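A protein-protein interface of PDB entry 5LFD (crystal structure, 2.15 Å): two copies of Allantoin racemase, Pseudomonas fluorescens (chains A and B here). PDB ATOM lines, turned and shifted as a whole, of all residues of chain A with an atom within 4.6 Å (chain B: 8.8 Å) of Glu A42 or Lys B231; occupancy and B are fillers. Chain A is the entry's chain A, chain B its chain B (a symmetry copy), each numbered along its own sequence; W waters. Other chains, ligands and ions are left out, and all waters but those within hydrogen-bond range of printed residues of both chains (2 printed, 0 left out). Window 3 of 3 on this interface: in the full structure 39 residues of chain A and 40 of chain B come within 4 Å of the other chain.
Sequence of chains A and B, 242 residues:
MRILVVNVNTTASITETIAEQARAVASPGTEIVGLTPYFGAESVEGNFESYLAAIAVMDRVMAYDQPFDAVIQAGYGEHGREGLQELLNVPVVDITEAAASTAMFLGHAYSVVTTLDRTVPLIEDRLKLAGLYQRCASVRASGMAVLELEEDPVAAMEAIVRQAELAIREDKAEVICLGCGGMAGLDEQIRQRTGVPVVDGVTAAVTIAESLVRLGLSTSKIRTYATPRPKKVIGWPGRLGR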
ATOM      1  N   ASN A   9      34.858 -29.175  -8.604  1.00  0.00           N
ATOM      2  CA  ASN A   9      34.391 -28.979  -7.228  1.00  0.00           C
ATOM      3  C   ASN A   9      35.591 -28.977  -6.277  1.00  0.00           C
ATOM      4  O   ASN A   9      36.681 -29.311  -6.689  1.00  0.00           O
ATOM      5  CB  ASN A   9      33.294 -29.980  -6.816  1.00  0.00           C
ATOM      6  CG  ASN A   9      33.781 -31.434  -6.757  1.00  0.00           C
ATOM      7  OD1 ASN A   9      34.753 -31.781  -6.053  1.00  0.00           O
ATOM      8  ND2 ASN A   9      33.052 -32.309  -7.437  1.00  0.00           N
ATOM      9  N   THR A  10      35.366 -28.626  -5.017  1.00  0.00           N
ATOM     10  CA  THR A  10      36.442 -28.393  -4.058  1.00  0.00           C
ATOM     11  C   THR A  10      36.777 -29.630  -3.200  1.00  0.00           C
ATOM     12  O   THR A  10      37.545 -29.512  -2.270  1.00  0.00           O
ATOM     13  CB  THR A  10      36.066 -27.206  -3.139  1.00  0.00           C
ATOM     14  OG1 THR A  10      34.821 -27.493  -2.491  1.00  0.00           O
ATOM     15  CG2 THR A  10      35.926 -25.898  -3.945  1.00  0.00           C
ATOM     16  N   THR A  11      36.240 -30.808  -3.515  1.00  0.00           N
ATOM     17  CA  THR A  11      36.461 -31.985  -2.674  1.00  0.00           C
ATOM     18  C   THR A  11      37.740 -32.650  -3.110  1.00  0.00           C
ATOM     19  O   THR A  11      37.783 -33.227  -4.184  1.00  0.00           O
ATOM     20  CB  THR A  11      35.355 -33.045  -2.814  1.00  0.00           C
ATOM     21  OG1 THR A  11      34.064 -32.465  -2.636  1.00  0.00           O
ATOM     22  CG2 THR A  11      35.528 -34.086  -1.775  1.00  0.00           C
ATOM     23  N   GLY A  40      34.407 -22.480  -4.224  1.00  0.00           N
ATOM     24  CA  GLY A  40      33.309 -23.120  -4.964  1.00  0.00           C
ATOM     25  C   GLY A  40      32.643 -24.226  -4.164  1.00  0.00           C
ATOM     26  O   GLY A  40      33.079 -24.564  -3.038  1.00  0.00           O
ATOM     27  N   ALA A  41      31.593 -24.779  -4.746  1.00  0.00           N
ATOM     28  CA  ALA A  41      30.790 -25.843  -4.138  1.00  0.00           C
ATOM     29  C   ALA A  41      31.548 -27.171  -4.069  1.00  0.00           C
ATOM     30  O   ALA A  41      32.300 -27.511  -4.992  1.00  0.00           O
ATOM     31  CB  ALA A  41      29.508 -26.046  -4.939  1.00  0.00           C
ATOM     32  N   GLU A  42      31.288 -27.931  -3.007  1.00  0.00           N
ATOM     33  CA  GLU A  42      31.914 -29.238  -2.764  1.00  0.00           C
ATOM     34  C   GLU A  42      31.453 -30.307  -3.787  1.00  0.00           C
ATOM     35  O   GLU A  42      32.124 -31.335  -3.991  1.00  0.00           O
ATOM     36  CB  GLU A  42      31.576 -29.683  -1.350  1.00  0.00           C
ATOM     37  CG  GLU A  42      30.097 -29.940  -1.121  1.00  0.00           C
ATOM     38  CD  GLU A  42      29.836 -30.598   0.222  1.00  0.00           C
ATOM     39  OE1 GLU A  42      30.746 -31.310   0.738  1.00  0.00           O
ATOM     40  OE2 GLU A  42      28.732 -30.393   0.763  1.00  0.00           O
ATOM     41  N   SER A  43      30.307 -30.053  -4.410  1.00  0.00           N
ATOM     42  CA  SER A  43      29.890 -30.741  -5.656  1.00  0.00           C
ATOM     43  C   SER A  43      29.031 -29.750  -6.476  1.00  0.00           C
ATOM     44  O   SER A  43      28.242 -29.024  -5.906  1.00  0.00           O
ATOM     45  CB  SER A  43      29.114 -32.047  -5.364  1.00  0.00           C
ATOM     46  OG  SER A  43      27.790 -31.761  -5.012  1.00  0.00           O
ATOM     47  N   GLU A  45      26.249 -28.619  -8.742  1.00  0.00           N
ATOM     48  CA  GLU A  45      24.942 -29.148  -9.159  1.00  0.00           C
ATOM     49  C   GLU A  45      24.003 -28.007  -9.537  1.00  0.00           C
ATOM     50  O   GLU A  45      23.250 -27.509  -8.692  1.00  0.00           O
ATOM     51  CB  GLU A  45      24.316 -30.008  -8.056  1.00  0.00           C
ATOM     52  CG  GLU A  45      25.321 -30.883  -7.284  1.00  0.00           C
ATOM     53  CD  GLU A  45      24.678 -31.625  -6.105  1.00  0.00           C
ATOM     54  OE1 GLU A  45      23.738 -31.089  -5.482  1.00  0.00           O
ATOM     55  OE2 GLU A  45      25.105 -32.760  -5.813  1.00  0.00           O
ATOM     56  N   GLU A  49      26.221 -22.907  -9.251  1.00  0.00           N
ATOM     57  CA  GLU A  49      27.470 -23.570  -8.869  1.00  0.00           C
ATOM     58  C   GLU A  49      28.332 -23.856 -10.098  1.00  0.00           C
ATOM     59  O   GLU A  49      29.548 -23.886  -9.977  1.00  0.00           O
ATOM     60  CB  GLU A  49      27.164 -24.834  -8.076  1.00  0.00           C
ATOM     61  CG  GLU A  49      26.356 -24.553  -6.800  1.00  0.00           C
ATOM     62  CD  GLU A  49      25.864 -25.800  -6.104  1.00  0.00           C
ATOM     63  OE1 GLU A  49      26.035 -26.908  -6.648  1.00  0.00           O
ATOM     64  OE2 GLU A  49      25.291 -25.687  -4.998  1.00  0.00           O
ATOM     65  N   LEU A 147      28.052 -37.297  -4.063  1.00  0.00           N
ATOM     66  CA  LEU A 147      28.889 -37.871  -3.001  1.00  0.00           C
ATOM     67  C   LEU A 147      28.469 -39.290  -2.524  1.00  0.00           C
ATOM     68  O   LEU A 147      29.279 -40.005  -1.922  1.00  0.00           O
ATOM     69  CB  LEU A 147      29.032 -36.871  -1.833  1.00  0.00           C
ATOM     70  CG  LEU A 147      29.307 -35.375  -2.151  1.00  0.00           C
ATOM     71  CD1 LEU A 147      28.918 -34.489  -0.971  1.00  0.00           C
ATOM     72  CD2 LEU A 147      30.728 -35.053  -2.619  1.00  0.00           C
ATOM     73  N   THR B 227      15.934 -24.083  -6.572  1.00  0.00           N
ATOM     74  CA  THR B 227      16.858 -23.512  -5.612  1.00  0.00           C
ATOM     75  C   THR B 227      18.051 -24.466  -5.420  1.00  0.00           C
ATOM     76  O   THR B 227      17.875 -25.710  -5.338  1.00  0.00           O
ATOM     77  CB  THR B 227      16.168 -23.322  -4.249  1.00  0.00           C
ATOM     78  OG1 THR B 227      14.935 -22.661  -4.474  1.00  0.00           O
ATOM     79  CG2 THR B 227      17.056 -22.437  -3.253  1.00  0.00           C
ATOM     80  N   PRO B 228      19.252 -23.896  -5.367  1.00  0.00           N
ATOM     81  CA  PRO B 228      20.410 -24.759  -5.208  1.00  0.00           C
ATOM     82  C   PRO B 228      20.299 -25.527  -3.856  1.00  0.00           C
ATOM     83  O   PRO B 228      19.812 -24.961  -2.814  1.00  0.00           O
ATOM     84  CB  PRO B 228      21.609 -23.796  -5.289  1.00  0.00           C
ATOM     85  CG  PRO B 228      21.081 -22.506  -5.884  1.00  0.00           C
ATOM     86  CD  PRO B 228      19.603 -22.472  -5.523  1.00  0.00           C
ATOM     87  N   ARG B 229      20.635 -26.823  -3.899  1.00  0.00           N
ATOM     88  CA  ARG B 229      20.605 -27.666  -2.700  1.00  0.00           C
ATOM     89  C   ARG B 229      21.640 -27.120  -1.696  1.00  0.00           C
ATOM     90  O   ARG B 229      22.832 -27.052  -2.030  1.00  0.00           O
ATOM     91  CB  ARG B 229      20.929 -29.105  -3.047  1.00  0.00           C
ATOM     92  CG  ARG B 229      21.026 -29.985  -1.809  1.00  0.00           C
ATOM     93  CD  ARG B 229      21.330 -31.442  -2.120  1.00  0.00           C
ATOM     94  NE  ARG B 229      22.681 -31.662  -2.671  1.00  0.00           N
ATOM     95  CZ  ARG B 229      23.789 -31.819  -1.939  1.00  0.00           C
ATOM     96  NH1 ARG B 229      23.763 -31.775  -0.585  1.00  0.00           N
ATOM     97  NH2 ARG B 229      24.944 -31.980  -2.558  1.00  0.00           N
ATOM     98  N   PRO B 230      21.192 -26.710  -0.475  1.00  0.00           N
ATOM     99  CA  PRO B 230      22.147 -26.093   0.474  1.00  0.00           C
ATOM    100  C   PRO B 230      23.223 -27.112   0.787  1.00  0.00           C
ATOM    101  O   PRO B 230      22.905 -28.289   1.027  1.00  0.00           O
ATOM    102  CB  PRO B 230      21.290 -25.789   1.714  1.00  0.00           C
ATOM    103  CG  PRO B 230      19.863 -25.814   1.193  1.00  0.00           C
ATOM    104  CD  PRO B 230      19.867 -26.898   0.148  1.00  0.00           C
ATOM    105  N   LYS B 231      24.483 -26.672   0.703  1.00  0.00           N
ATOM    106  CA  LYS B 231      25.621 -27.560   0.846  1.00  0.00           C
ATOM    107  C   LYS B 231      26.826 -26.693   1.182  1.00  0.00           C
ATOM    108  O   LYS B 231      26.708 -25.477   1.293  1.00  0.00           O
ATOM    109  CB  LYS B 231      25.871 -28.303  -0.481  1.00  0.00           C
ATOM    110  CG  LYS B 231      26.244 -27.346  -1.598  1.00  0.00           C
ATOM    111  CD  LYS B 231      26.454 -28.071  -2.906  1.00  0.00           C
ATOM    112  CE  LYS B 231      25.146 -28.455  -3.570  1.00  0.00           C
ATOM    113  NZ  LYS B 231      25.634 -29.348  -4.628  1.00  0.00           N
ATOM    114  N   LYS B 232      27.997 -27.312   1.284  1.00  0.00           N
ATOM    115  CA  LYS B 232      29.227 -26.607   1.627  1.00  0.00           C
ATOM    116  C   LYS B 232      29.737 -25.902   0.385  1.00  0.00           C
ATOM    117  O   LYS B 232      30.059 -26.533  -0.642  1.00  0.00           O
ATOM    118  CB  LYS B 232      30.301 -27.614   2.137  1.00  0.00           C
ATOM    119  CG  LYS B 232      31.569 -26.915   2.664  1.00  0.00           C
ATOM    120  CD  LYS B 232      32.917 -27.387   2.081  1.00  0.00           C
ATOM    121  CE  LYS B 232      33.802 -28.078   3.121  1.00  0.00           C
ATOM    122  NZ  LYS B 232      33.763 -27.440   4.479  1.00  0.00           N
ATOM    123  N   VAL B 233      29.766 -24.586   0.440  1.00  0.00           N
ATOM    124  CA  VAL B 233      30.398 -23.827  -0.612  1.00  0.00           C
ATOM    125  C   VAL B 233      31.335 -22.853   0.031  1.00  0.00           C
ATOM    126  O   VAL B 233      31.014 -22.285   1.073  1.00  0.00           O
ATOM    127  CB  VAL B 233      29.406 -23.262  -1.722  1.00  0.00           C
ATOM    128  CG1 VAL B 233      27.962 -23.324  -1.331  1.00  0.00           C
ATOM    129  CG2 VAL B 233      29.797 -21.921  -2.309  1.00  0.00           C
ATOM    130  N   ILE B 234      32.515 -22.713  -0.573  1.00  0.00           N
ATOM    131  CA  ILE B 234      33.584 -21.852  -0.083  1.00  0.00           C
ATOM    132  C   ILE B 234      33.669 -20.587  -0.906  1.00  0.00           C
ATOM    133  O   ILE B 234      33.540 -20.645  -2.140  1.00  0.00           O
ATOM    134  CB  ILE B 234      34.959 -22.564  -0.159  1.00  0.00           C
ATOM    135  CG1 ILE B 234      34.999 -23.779   0.763  1.00  0.00           C
ATOM    136  CG2 ILE B 234      36.089 -21.611   0.198  1.00  0.00           C
ATOM    137  CD1 ILE B 234      36.243 -24.629   0.558  1.00  0.00           C
HETATM  138  O   HOH W   1      26.464 -32.607   0.443  1.00  0.00           O
HETATM  139  O   HOH W   2      22.227 -27.605  -6.348  1.00  0.00           O
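No position is printed for both chains.
Of the 11 pairs that touch across the chains among the printed residues, none has its exchanged pair printed and touching as well.
The backbone carbonyl oxygen of Glu A42 lies within hydrogen-bond range of the side-chain hydroxyl of Thr A11.
The side-chain hydroxyl (OG1) of Thr A10 sits close to the backbone carbonyl oxygen (O) of Gly A40 (3.5 Å).
The backbone NH of Glu A45 lies within hydrogen-bond range of the side-chain carboxylate of Glu A49 (2.7 Å).
O of Ala A41 sits at hydrogen-bond distance from N of Thr A10 (3.3 Å).
The side-chain amide oxygen (OD1) of Asn A9 sits close to the backbone carbonyl oxygen (O) of Glu A42, at 3.4 Å.
The side-chain hydroxyl of Ser A43 sits at hydrogen-bond distance from the side-chain carboxylate of Glu A45 (3.0 Å).
Water W2 lies within hydrogen-bond range of the backbone carbonyl oxygen (O) of Glu A45 (2.6 Å) and the backbone NH (N) of Arg B229 (3.0 Å).
Water W1 bridges the guanidinium group of Arg B229 (3.0 Å) and the side-chain carboxylate of Glu A42 (3.2 Å).
Printed residues of chain B within 4 Å of Gly A40: Val B233 and Ile B234.
Ala A41 touches two residues of chain B.
Glu A42 touches just these residues of chain B: Lys B231 (3.8 Å) and Lys B232 (3.0 Å).
Ser A43 touches two residues of chain B.
Printed residues of chain B within 4 Å of Glu A45: Arg B229 and Lys B231.
Lys B231 touches four residues of chain A.
Of the printed residues of chain A, Lys B232 touches Ala A41 and Glu A42.
Printed residues of chain A within 4 Å of Val B233: Gly A40 (3.7 Å) and Ala A41 (3.8 Å).
Printed residues of chain A within 4 Å of Ile B234: Gly A40.
The nearest residue of chain B that does not touch Glu A42 is Val B233 (4.8 Å).
The nearest printed residue of chain A that does not touch Lys B232 is Gly A40 (4.3 Å).
Of the 8 printed residues of chain B, 5 touch a printed residue of chain A.
Printed residues of chain B that touch a printed residue of chain A: Arg B229, Lys B231, Lys B232, Val B233 and Ile B234.
Hydrophobic or aromatic side chains of chain B that line the printed part of chain A: Val B233 and Ile B234.
Among the printed residues, 11 pairs touch across the chains.
OE1 of Glu A49 is in salt-bridge range of NZ of Lys B231.
The side-chain carboxylate (OE1) of Glu A45 is in salt-bridge range of the side-chain amino group (NZ) of Lys B231 (2.7 Å).
The backbone carbonyl oxygen of Ser A43 sits at hydrogen-bond distance from the side-chain amino group of Lys B231, at 2.9 Å.
The backbone carbonyl oxygen (O) of Lys B232 is in hydrogen-bond range of the backbone NH (N) of Glu A42 (3.0 Å).
The backbone carbonyl oxygen of Ile B234 lies within hydrogen-bond range of the backbone NH of Gly A40 (2.9 Å).
The guanidinium group (NE) of Arg B229 lies within salt-bridge range of the side-chain carboxylate (OE1) of Glu A45, 3.1 Å away.
Among the printed residues, pairs that only touch across the chains: Ala A41 with Lys B232 (3.6 Å), Gly A40 with Val B233 (3.7 Å), Glu A42 with Lys B231 (3.8 Å), Ser A43 with Arg B229 (3.8 Å) and Ala A41 with Val B233 (3.8 Å).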
